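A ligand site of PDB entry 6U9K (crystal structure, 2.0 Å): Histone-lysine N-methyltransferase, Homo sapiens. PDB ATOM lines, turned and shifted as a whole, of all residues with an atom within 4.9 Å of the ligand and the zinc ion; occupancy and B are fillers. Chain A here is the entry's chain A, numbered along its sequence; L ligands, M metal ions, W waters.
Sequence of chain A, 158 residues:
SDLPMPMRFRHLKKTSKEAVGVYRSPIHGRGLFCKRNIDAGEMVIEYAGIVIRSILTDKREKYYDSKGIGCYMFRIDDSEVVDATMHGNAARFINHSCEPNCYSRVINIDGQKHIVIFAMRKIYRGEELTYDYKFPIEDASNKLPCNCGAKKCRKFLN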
ATOM      1  N   ILE A  27      15.938  -8.445  31.533  1.00  0.00           N
ATOM      2  CA  ILE A  27      16.845  -8.485  30.379  1.00  0.00           C
ATOM      3  C   ILE A  27      16.230  -9.477  29.365  1.00  0.00           C
ATOM      4  O   ILE A  27      15.890  -9.069  28.257  1.00  0.00           O
ATOM      5  CB  ILE A  27      18.307  -8.850  30.787  1.00  0.00           C
ATOM      6  CG1 ILE A  27      18.957  -7.732  31.627  1.00  0.00           C
ATOM      7  CG2 ILE A  27      19.144  -9.133  29.526  1.00  0.00           C
ATOM      8  CD1 ILE A  27      20.250  -8.177  32.458  1.00  0.00           C
ATOM      9  N   HIS A  28      16.062 -10.746  29.772  1.00  0.00           N
ATOM     10  CA  HIS A  28      15.444 -11.793  28.955  1.00  0.00           C
ATOM     11  C   HIS A  28      15.016 -12.974  29.814  1.00  0.00           C
ATOM     12  O   HIS A  28      15.826 -13.474  30.609  1.00  0.00           O
ATOM     13  CB  HIS A  28      16.399 -12.260  27.839  1.00  0.00           C
ATOM     14  CG  HIS A  28      15.864 -13.385  27.005  1.00  0.00           C
ATOM     15  ND1 HIS A  28      15.884 -14.701  27.463  1.00  0.00           N
ATOM     16  CD2 HIS A  28      15.354 -13.365  25.754  1.00  0.00           C
ATOM     17  CE1 HIS A  28      15.343 -15.420  26.499  1.00  0.00           C
ATOM     18  NE2 HIS A  28      15.049 -14.666  25.439  1.00  0.00           N
ATOM     19  N   GLY A  29      13.796 -13.477  29.554  1.00  0.00           N
ATOM     20  CA  GLY A  29      13.209 -14.683  30.150  1.00  0.00           C
ATOM     21  C   GLY A  29      13.502 -14.868  31.617  1.00  0.00           C
ATOM     22  O   GLY A  29      12.987 -14.128  32.454  1.00  0.00           O
ATOM     23  N   ARG A  30      14.362 -15.850  31.946  1.00  0.00           N
ATOM     24  CA  ARG A  30      14.788 -16.038  33.340  1.00  0.00           C
ATOM     25  C   ARG A  30      16.270 -15.703  33.449  1.00  0.00           C
ATOM     26  O   ARG A  30      16.992 -15.789  32.468  1.00  0.00           O
ATOM     27  CB  ARG A  30      14.510 -17.470  33.853  1.00  0.00           C
ATOM     28  CG  ARG A  30      12.998 -17.718  34.138  1.00  0.00           C
ATOM     29  CD  ARG A  30      12.726 -19.026  34.866  1.00  0.00           C
ATOM     30  NE  ARG A  30      12.929 -20.185  34.000  1.00  0.00           N
ATOM     31  CZ  ARG A  30      12.900 -21.452  34.417  1.00  0.00           C
ATOM     32  NH1 ARG A  30      12.710 -21.729  35.697  1.00  0.00           N
ATOM     33  NH2 ARG A  30      13.100 -22.449  33.562  1.00  0.00           N
ATOM     34  N   GLY A  68      11.340 -29.281  21.222  1.00  0.00           N
ATOM     35  CA  GLY A  68      10.839 -28.126  21.969  1.00  0.00           C
ATOM     36  C   GLY A  68      11.501 -27.988  23.338  1.00  0.00           C
ATOM     37  O   GLY A  68      10.865 -27.532  24.288  1.00  0.00           O
ATOM     38  N   ILE A  69      12.766 -28.410  23.433  1.00  0.00           N
ATOM     39  CA  ILE A  69      13.609 -28.355  24.641  1.00  0.00           C
ATOM     40  C   ILE A  69      14.577 -27.192  24.459  1.00  0.00           C
ATOM     41  O   ILE A  69      15.277 -27.161  23.445  1.00  0.00           O
ATOM     42  CB  ILE A  69      14.391 -29.699  24.819  1.00  0.00           C
ATOM     43  CG1 ILE A  69      13.444 -30.889  25.105  1.00  0.00           C
ATOM     44  CG2 ILE A  69      15.492 -29.599  25.888  1.00  0.00           C
ATOM     45  CD1 ILE A  69      14.101 -32.294  24.871  1.00  0.00           C
ATOM     46  N   GLY A  70      14.634 -26.296  25.450  1.00  0.00           N
ATOM     47  CA  GLY A  70      15.567 -25.165  25.433  1.00  0.00           C
ATOM     48  C   GLY A  70      16.996 -25.695  25.360  1.00  0.00           C
ATOM     49  O   GLY A  70      17.325 -26.641  26.069  1.00  0.00           O
ATOM     50  N   CYS A  71      17.826 -25.126  24.472  1.00  0.00           N
ATOM     51  CA  CYS A  71      19.226 -25.513  24.233  1.00  0.00           C
ATOM     52  C   CYS A  71      20.126 -24.573  25.008  1.00  0.00           C
ATOM     53  O   CYS A  71      20.153 -23.395  24.704  1.00  0.00           O
ATOM     54  CB  CYS A  71      19.527 -25.465  22.729  1.00  0.00           C
ATOM     55  SG  CYS A  71      21.235 -25.890  22.308  1.00  0.00           S
ATOM     56  N   TYR A  72      20.881 -25.087  25.987  1.00  0.00           N
ATOM     57  CA  TYR A  72      21.753 -24.258  26.845  1.00  0.00           C
ATOM     58  C   TYR A  72      23.176 -24.632  26.596  1.00  0.00           C
ATOM     59  O   TYR A  72      23.585 -25.699  27.015  1.00  0.00           O
ATOM     60  CB  TYR A  72      21.384 -24.473  28.345  1.00  0.00           C
ATOM     61  CG  TYR A  72      20.021 -23.913  28.705  1.00  0.00           C
ATOM     62  CD1 TYR A  72      19.884 -22.622  29.209  1.00  0.00           C
ATOM     63  CD2 TYR A  72      18.858 -24.657  28.474  1.00  0.00           C
ATOM     64  CE1 TYR A  72      18.634 -22.097  29.515  1.00  0.00           C
ATOM     65  CE2 TYR A  72      17.589 -24.114  28.732  1.00  0.00           C
ATOM     66  CZ  TYR A  72      17.487 -22.819  29.225  1.00  0.00           C
ATOM     67  OH  TYR A  72      16.265 -22.242  29.474  1.00  0.00           O
ATOM     68  N   ARG A  92      23.227 -21.877  33.864  1.00  0.00           N
ATOM     69  CA  ARG A  92      22.786 -21.865  32.460  1.00  0.00           C
ATOM     70  C   ARG A  92      21.819 -20.725  32.149  1.00  0.00           C
ATOM     71  O   ARG A  92      21.612 -20.427  30.981  1.00  0.00           O
ATOM     72  CB  ARG A  92      22.231 -23.234  32.002  1.00  0.00           C
ATOM     73  CG  ARG A  92      20.834 -23.577  32.474  1.00  0.00           C
ATOM     74  CD  ARG A  92      20.538 -25.056  32.143  1.00  0.00           C
ATOM     75  NE  ARG A  92      19.169 -25.442  32.463  1.00  0.00           N
ATOM     76  CZ  ARG A  92      18.755 -25.852  33.665  1.00  0.00           C
ATOM     77  NH1 ARG A  92      19.607 -25.901  34.680  1.00  0.00           N
ATOM     78  NH2 ARG A  92      17.494 -26.205  33.855  1.00  0.00           N
ATOM     79  N   PHE A  93      21.238 -20.074  33.191  1.00  0.00           N
ATOM     80  CA  PHE A  93      20.320 -18.958  32.995  1.00  0.00           C
ATOM     81  C   PHE A  93      21.021 -17.596  33.031  1.00  0.00           C
ATOM     82  O   PHE A  93      20.342 -16.572  32.913  1.00  0.00           O
ATOM     83  CB  PHE A  93      19.185 -18.996  34.028  1.00  0.00           C
ATOM     84  CG  PHE A  93      18.332 -20.251  33.917  1.00  0.00           C
ATOM     85  CD1 PHE A  93      17.320 -20.340  32.961  1.00  0.00           C
ATOM     86  CD2 PHE A  93      18.540 -21.330  34.770  1.00  0.00           C
ATOM     87  CE1 PHE A  93      16.535 -21.493  32.855  1.00  0.00           C
ATOM     88  CE2 PHE A  93      17.731 -22.471  34.681  1.00  0.00           C
ATOM     89  CZ  PHE A  93      16.737 -22.546  33.723  1.00  0.00           C
ATOM     90  N   ILE A  94      22.347 -17.561  33.187  1.00  0.00           N
ATOM     91  CA  ILE A  94      23.070 -16.287  33.250  1.00  0.00           C
ATOM     92  C   ILE A  94      22.951 -15.529  31.938  1.00  0.00           C
ATOM     93  O   ILE A  94      23.408 -16.023  30.912  1.00  0.00           O
ATOM     94  CB  ILE A  94      24.558 -16.393  33.738  1.00  0.00           C
ATOM     95  CG1 ILE A  94      24.659 -17.038  35.128  1.00  0.00           C
ATOM     96  CG2 ILE A  94      25.213 -14.982  33.764  1.00  0.00           C
ATOM     97  CD1 ILE A  94      26.101 -17.545  35.514  1.00  0.00           C
ATOM     98  N   ASN A  95      22.378 -14.340  32.003  1.00  0.00           N
ATOM     99  CA  ASN A  95      22.176 -13.455  30.855  1.00  0.00           C
ATOM    100  C   ASN A  95      23.405 -12.611  30.559  1.00  0.00           C
ATOM    101  O   ASN A  95      24.273 -12.446  31.402  1.00  0.00           O
ATOM    102  CB  ASN A  95      20.945 -12.548  31.085  1.00  0.00           C
ATOM    103  CG  ASN A  95      19.626 -13.261  30.859  1.00  0.00           C
ATOM    104  OD1 ASN A  95      19.493 -14.093  29.949  1.00  0.00           O
ATOM    105  ND2 ASN A  95      18.615 -12.934  31.656  1.00  0.00           N
ATOM    106  N   HIS A  96      23.473 -12.089  29.329  1.00  0.00           N
ATOM    107  CA  HIS A  96      24.551 -11.210  28.870  1.00  0.00           C
ATOM    108  C   HIS A  96      24.340  -9.767  29.339  1.00  0.00           C
ATOM    109  O   HIS A  96      23.196  -9.304  29.390  1.00  0.00           O
ATOM    110  CB  HIS A  96      24.619 -11.196  27.310  1.00  0.00           C
ATOM    111  CG  HIS A  96      25.481 -10.101  26.775  1.00  0.00           C
ATOM    112  ND1 HIS A  96      26.847 -10.225  26.723  1.00  0.00           N
ATOM    113  CD2 HIS A  96      25.143  -8.844  26.395  1.00  0.00           C
ATOM    114  CE1 HIS A  96      27.302  -9.068  26.280  1.00  0.00           C
ATOM    115  NE2 HIS A  96      26.317  -8.199  26.087  1.00  0.00           N
ATOM    116  N   SER A  97      25.443  -9.040  29.591  1.00  0.00           N
ATOM    117  CA  SER A  97      25.431  -7.593  29.869  1.00  0.00           C
ATOM    118  C   SER A  97      26.698  -6.953  29.388  1.00  0.00           C
ATOM    119  O   SER A  97      27.759  -7.578  29.453  1.00  0.00           O
ATOM    120  CB  SER A  97      25.232  -7.285  31.346  1.00  0.00           C
ATOM    121  OG  SER A  97      25.260  -5.882  31.561  1.00  0.00           O
ATOM    122  N   CYS A  98      26.596  -5.662  28.947  1.00  0.00           N
ATOM    123  CA  CYS A  98      27.720  -4.874  28.441  1.00  0.00           C
ATOM    124  C   CYS A  98      28.446  -4.176  29.568  1.00  0.00           C
ATOM    125  O   CYS A  98      29.561  -3.670  29.376  1.00  0.00           O
ATOM    126  CB  CYS A  98      27.257  -3.907  27.360  1.00  0.00           C
ATOM    127  SG  CYS A  98      26.345  -4.705  26.020  1.00  0.00           S
ATOM    128  N   TYR A 133      28.928 -12.113  26.947  1.00  0.00           N
ATOM    129  CA  TYR A 133      28.947 -13.289  26.063  1.00  0.00           C
ATOM    130  C   TYR A 133      30.036 -13.083  25.002  1.00  0.00           C
ATOM    131  O   TYR A 133      30.156 -11.971  24.486  1.00  0.00           O
ATOM    132  CB  TYR A 133      27.595 -13.464  25.345  1.00  0.00           C
ATOM    133  CG  TYR A 133      26.441 -14.033  26.158  1.00  0.00           C
ATOM    134  CD1 TYR A 133      26.508 -14.133  27.546  1.00  0.00           C
ATOM    135  CD2 TYR A 133      25.257 -14.425  25.543  1.00  0.00           C
ATOM    136  CE1 TYR A 133      25.445 -14.653  28.292  1.00  0.00           C
ATOM    137  CE2 TYR A 133      24.177 -14.904  26.278  1.00  0.00           C
ATOM    138  CZ  TYR A 133      24.280 -15.023  27.648  1.00  0.00           C
ATOM    139  OH  TYR A 133      23.227 -15.533  28.345  1.00  0.00           O
ATOM    140  N   PHE A 135      30.359 -13.545  21.935  1.00  0.00           N
ATOM    141  CA  PHE A 135      29.880 -13.007  20.664  1.00  0.00           C
ATOM    142  C   PHE A 135      29.207 -11.651  20.816  1.00  0.00           C
ATOM    143  O   PHE A 135      29.243 -10.846  19.891  1.00  0.00           O
ATOM    144  CB  PHE A 135      28.940 -14.023  19.967  1.00  0.00           C
ATOM    145  CG  PHE A 135      27.690 -14.416  20.723  1.00  0.00           C
ATOM    146  CD1 PHE A 135      27.745 -15.348  21.757  1.00  0.00           C
ATOM    147  CD2 PHE A 135      26.445 -13.922  20.347  1.00  0.00           C
ATOM    148  CE1 PHE A 135      26.582 -15.738  22.438  1.00  0.00           C
ATOM    149  CE2 PHE A 135      25.281 -14.311  21.028  1.00  0.00           C
ATOM    150  CZ  PHE A 135      25.365 -15.214  22.065  1.00  0.00           C
ATOM    151  N   PRO A 145      19.701  -8.172  19.228  1.00  0.00           N
ATOM    152  CA  PRO A 145      19.747  -6.913  20.001  1.00  0.00           C
ATOM    153  C   PRO A 145      19.927  -7.109  21.509  1.00  0.00           C
ATOM    154  O   PRO A 145      19.334  -8.033  22.070  1.00  0.00           O
ATOM    155  CB  PRO A 145      18.410  -6.228  19.661  1.00  0.00           C
ATOM    156  CG  PRO A 145      17.527  -7.324  19.152  1.00  0.00           C
ATOM    157  CD  PRO A 145      18.432  -8.304  18.477  1.00  0.00           C
ATOM    158  N   CYS A 146      20.781  -6.294  22.154  1.00  0.00           N
ATOM    159  CA  CYS A 146      21.041  -6.392  23.586  1.00  0.00           C
ATOM    160  C   CYS A 146      20.053  -5.604  24.396  1.00  0.00           C
ATOM    161  O   CYS A 146      19.791  -4.425  24.088  1.00  0.00           O
ATOM    162  CB  CYS A 146      22.471  -6.001  23.930  1.00  0.00           C
ATOM    163  SG  CYS A 146      22.933  -6.362  25.637  1.00  0.00           S
ATOM    164  N   ASN A 147      19.567  -6.205  25.491  1.00  0.00           N
ATOM    165  CA  ASN A 147      18.591  -5.612  26.399  1.00  0.00           C
ATOM    166  C   ASN A 147      19.162  -5.444  27.829  1.00  0.00           C
ATOM    167  O   ASN A 147      18.395  -5.398  28.795  1.00  0.00           O
ATOM    168  CB  ASN A 147      17.297  -6.446  26.398  1.00  0.00           C
ATOM    169  CG  ASN A 147      16.066  -5.709  26.895  1.00  0.00           C
ATOM    170  OD1 ASN A 147      15.823  -4.539  26.578  1.00  0.00           O
ATOM    171  ND2 ASN A 147      15.262  -6.387  27.686  1.00  0.00           N
ATOM    172  N   CYS A 148      20.499  -5.335  27.964  1.00  0.00           N
ATOM    173  CA  CYS A 148      21.124  -5.169  29.293  1.00  0.00           C
ATOM    174  C   CYS A 148      20.786  -3.806  29.915  1.00  0.00           C
ATOM    175  O   CYS A 148      20.764  -3.687  31.148  1.00  0.00           O
ATOM    176  CB  CYS A 148      22.630  -5.427  29.233  1.00  0.00           C
ATOM    177  SG  CYS A 148      23.604  -4.055  28.552  1.00  0.00           S
ATOM    178  N   GLY A 149      20.532  -2.808  29.057  1.00  0.00           N
ATOM    179  CA  GLY A 149      20.155  -1.458  29.435  1.00  0.00           C
ATOM    180  C   GLY A 149      21.279  -0.578  29.934  1.00  0.00           C
ATOM    181  O   GLY A 149      21.014   0.541  30.384  1.00  0.00           O
ATOM    182  N   CYS A 153      26.152   0.288  26.535  1.00  0.00           N
ATOM    183  CA  CYS A 153      25.648  -0.892  25.835  1.00  0.00           C
ATOM    184  C   CYS A 153      26.136  -0.946  24.395  1.00  0.00           C
ATOM    185  O   CYS A 153      26.090   0.062  23.710  1.00  0.00           O
ATOM    186  CB  CYS A 153      24.120  -0.956  25.915  1.00  0.00           C
ATOM    187  SG  CYS A 153      23.383  -2.406  25.109  1.00  0.00           S
ATOM    188  N   ARG A 154      26.628  -2.133  23.940  1.00  0.00           N
ATOM    189  CA  ARG A 154      27.101  -2.353  22.569  1.00  0.00           C
ATOM    190  C   ARG A 154      25.912  -2.599  21.619  1.00  0.00           C
ATOM    191  O   ARG A 154      26.099  -2.745  20.427  1.00  0.00           O
ATOM    192  CB  ARG A 154      28.136  -3.500  22.512  1.00  0.00           C
ATOM    193  N   LYS A 155      24.689  -2.656  22.196  1.00  0.00           N
ATOM    194  CA  LYS A 155      23.378  -2.780  21.541  1.00  0.00           C
ATOM    195  C   LYS A 155      23.115  -4.107  20.814  1.00  0.00           C
ATOM    196  O   LYS A 155      21.980  -4.327  20.372  1.00  0.00           O
ATOM    197  CB  LYS A 155      23.109  -1.573  20.619  1.00  0.00           C
ATOM    198  CG  LYS A 155      23.240  -0.199  21.329  1.00  0.00           C
ATOM    199  CD  LYS A 155      22.185   0.058  22.412  1.00  0.00           C
ATOM    200  CE  LYS A 155      22.214   1.486  22.917  1.00  0.00           C
ATOM    201  NZ  LYS A 155      21.021   1.801  23.748  1.00  0.00           N
ATOM    202  N   LEU A 157      24.412  -8.600  20.875  1.00  0.00           N
ATOM    203  CA  LEU A 157      25.101  -9.720  21.505  1.00  0.00           C
ATOM    204  C   LEU A 157      26.167 -10.245  20.549  1.00  0.00           C
ATOM    205  O   LEU A 157      26.028 -10.081  19.338  1.00  0.00           O
ATOM    206  CB  LEU A 157      24.098 -10.834  21.832  1.00  0.00           C
ATOM    207  CG  LEU A 157      23.686 -10.979  23.291  1.00  0.00           C
ATOM    208  CD1 LEU A 157      22.908  -9.755  23.774  1.00  0.00           C
ATOM    209  CD2 LEU A 157      22.850 -12.228  23.487  1.00  0.00           C
HETATM  210  N1  LIG L   1      19.788  -9.064  25.641  1.00  0.00           N
HETATM  211  C1  LIG L   1      19.584 -11.783  25.876  1.00  0.00           C
HETATM  212  C2  LIG L   1      20.542 -11.111  26.686  1.00  0.00           C
HETATM  213  O1  LIG L   1      19.176 -15.411  26.254  1.00  0.00           O
HETATM  214  C3  LIG L   1      19.622 -14.455  24.078  1.00  0.00           C
HETATM  215  C4  LIG L   1      19.885 -16.362  25.486  1.00  0.00           C
HETATM  216  C5  LIG L   1      20.842 -17.109  26.439  1.00  0.00           C
HETATM  217  C6  LIG L   1      20.099 -19.359  27.317  1.00  0.00           C
HETATM  218  C7  LIG L   1      19.390 -19.720  25.990  1.00  0.00           C
HETATM  219  C8  LIG L   1      17.929 -19.175  25.791  1.00  0.00           C
HETATM  220  C9  LIG L   1      16.219 -21.033  25.994  1.00  0.00           C
HETATM  221  C10 LIG L   1      12.839 -19.197  26.121  1.00  0.00           C
HETATM  222  C11 LIG L   1      12.588 -18.565  24.887  1.00  0.00           C
HETATM  223  C12 LIG L   1      11.821 -17.402  24.834  1.00  0.00           C
HETATM  224  C13 LIG L   1      11.277 -16.850  26.012  1.00  0.00           C
HETATM  225  C14 LIG L   1      11.501 -17.484  27.236  1.00  0.00           C
HETATM  226  C15 LIG L   1      12.272 -18.653  27.295  1.00  0.00           C
HETATM  227  C16 LIG L   1      13.136 -21.684  25.817  1.00  0.00           C
HETATM  228  C17 LIG L   1      12.584 -22.511  26.818  1.00  0.00           C
HETATM  229  C18 LIG L   1      11.996 -23.748  26.487  1.00  0.00           C
HETATM  230  C19 LIG L   1      11.936 -24.167  25.151  1.00  0.00           C
HETATM  231  C20 LIG L   1      12.483 -23.357  24.138  1.00  0.00           C
HETATM  232  C21 LIG L   1      13.066 -22.114  24.463  1.00  0.00           C
HETATM  233  C22 LIG L   1      18.771 -21.099  25.947  1.00  0.00           C
HETATM  234  C23 LIG L   1      20.191 -17.336  28.863  1.00  0.00           C
HETATM  235  C24 LIG L   1      18.960 -17.740  29.757  1.00  0.00           C
HETATM  236  O2  LIG L   1      15.474 -17.834  30.171  1.00  0.00           O
HETATM  237  C25 LIG L   1      16.466 -18.120  29.549  1.00  0.00           C
HETATM  238  O3  LIG L   1      16.568 -19.390  29.130  1.00  0.00           O
HETATM  239  C26 LIG L   1      17.638 -17.203  29.159  1.00  0.00           C
HETATM  240  N2  LIG L   1      17.323 -15.884  29.718  1.00  0.00           N
HETATM  241  N3  LIG L   1      20.021 -17.874  27.476  1.00  0.00           N
HETATM  242  C27 LIG L   1      20.649 -15.565  24.365  1.00  0.00           C
HETATM  243  O4  LIG L   1      20.792 -16.335  23.234  1.00  0.00           O
HETATM  244  O5  LIG L   1      18.523 -14.863  23.338  1.00  0.00           O
HETATM  245  C28 LIG L   1      19.021 -14.224  25.526  1.00  0.00           C
HETATM  246  N4  LIG L   1      19.713 -13.126  26.193  1.00  0.00           N
HETATM  247  N5  LIG L   1      18.729 -11.176  24.977  1.00  0.00           N
HETATM  248  C29 LIG L   1      18.904  -9.836  24.932  1.00  0.00           C
HETATM  249  C30 LIG L   1      20.730 -13.218  27.184  1.00  0.00           C
HETATM  250  N6  LIG L   1      21.251 -12.014  27.493  1.00  0.00           N
HETATM  251  C31 LIG L   1      20.615  -9.696  26.523  1.00  0.00           C
HETATM  252  N7  LIG L   1      21.503  -8.948  27.254  1.00  0.00           N
HETATM  253  N8  LIG L   1      17.487 -20.549  25.377  1.00  0.00           N
HETATM  254  C32 LIG L   1      15.104 -20.076  25.521  1.00  0.00           C
HETATM  255  C33 LIG L   1      13.791 -20.379  26.255  1.00  0.00           C
HETATM  256 ZN    ZN M   1      24.119  -4.384  26.322  1.00  0.00          ZN
HETATM  257  O   HOH W   1      13.469 -19.437  30.888  1.00  0.00           O
HETATM  258  O   HOH W   2      17.302 -12.399  22.904  1.00  0.00           O
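Water W1 bridges an oxygen (O2) of the ligand (2.7 Å) and the guanidinium group (NE) of Arg 30 (3.2 Å).
Four residues have an atom within 4 Å of the zinc ion: Cys 98, Cys 146, Cys 148 and Cys 153.
The zinc ion is bound by SG of Cys 98, SG of Cys 148, SG of Cys 146 and SG of Cys 153. The zinc ion has four donor atoms within binding distance.
SG of Cys 146 sits close to N7 of the ligand, at 3.4 Å. N of His 96 is in hydrogen-bond range of N6 of the ligand, at 2.9 Å. O of His 96 is in hydrogen-bond range of N7 of the ligand (2.7 Å). The backbone NH (N) of Arg 30 is in hydrogen-bond range of an oxygen (O2) of the ligand, 2.9 Å away. The backbone carbonyl oxygen (O) of Arg 30 lies within hydrogen-bond range of a nitrogen (N2) of the ligand (2.8 Å). The side-chain amide oxygen of Asn 95 sits at hydrogen-bond distance from a nitrogen (N2) of the ligand, at 2.8 Å. N of Asn 147 sits at hydrogen-bond distance from N1 of the ligand. O3 of the ligand sits at hydrogen-bond distance from OH of Tyr 72 (2.9 Å). The backbone carbonyl oxygen (O) of His 28 sits at hydrogen-bond distance from a nitrogen (N2) of the ligand (3.0 Å). A ring nitrogen (ND1) of His 28 sits at hydrogen-bond distance from a nitrogen (N2) of the ligand (2.9 Å).
The side-chain sulfur of Cys 98 lies close to a ring nitrogen (NE2) of His 96, at 3.5 Å. SG of Cys 98 sits close to N of Arg 154 (3.3 Å). The backbone NH of Cys 146 lies within hydrogen-bond range of the backbone carbonyl oxygen of Lys 155 (2.9 Å). N of Lys 155 sits close to SG of Cys 153. A ring nitrogen (ND1) of His 96 is in hydrogen-bond range of the backbone NH (N) of Tyr 133, 2.8 Å away. ND2 of Asn 95 sits at hydrogen-bond distance from O of Arg 30 (3.4 Å). The side-chain amide nitrogen of Asn 147 sits at hydrogen-bond distance from the backbone carbonyl oxygen of Ile 27 (2.8 Å). The side-chain hydroxyl (OH) of Tyr 133 lies within hydrogen-bond range of the backbone carbonyl oxygen (O) of Ile 94.
Ile 27 touches the ligand (CG2 to N7, 3.3 Å). C of Gly 29 touches O2 of the ligand (3.8 Å). Gly 68 touches the ligand (O to C19, 3.6 Å). Gly 70 touches the ligand (N to C19, 3.4 Å). Cys 71 touches the ligand (O to C22, 3.0 Å). Arg 92 touches the ligand (O to C24, 3.97 Å). Phe 93 touches the ligand (O to C24, 3.6 Å). Tyr 133 touches the ligand (OH to C5, 3.4 Å). Pro 145 touches the ligand. Leu 157 touches the ligand (CD1 to C31, 3.6 Å). Hydrophobic or aromatic side chains that line the ligand: Ile 27, His 28, Tyr 72, His 96, Tyr 133 and Leu 157. 18 residues have an atom within 4 Å of the ligand: Ile 27, His 28, Gly 29, Arg 30, Gly 68, Gly 70, Cys 71, Tyr 72, Arg 92, Phe 93, Asn 95, His 96, Tyr 133, Pro 145, Cys 146, Asn 147, Cys 148 and Leu 157. Along chain A the residues within 4 Å of the ligand span positions 27 to 157. The nearest printed residue that does not touch the ligand is Ile 94 (4.03 Å).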
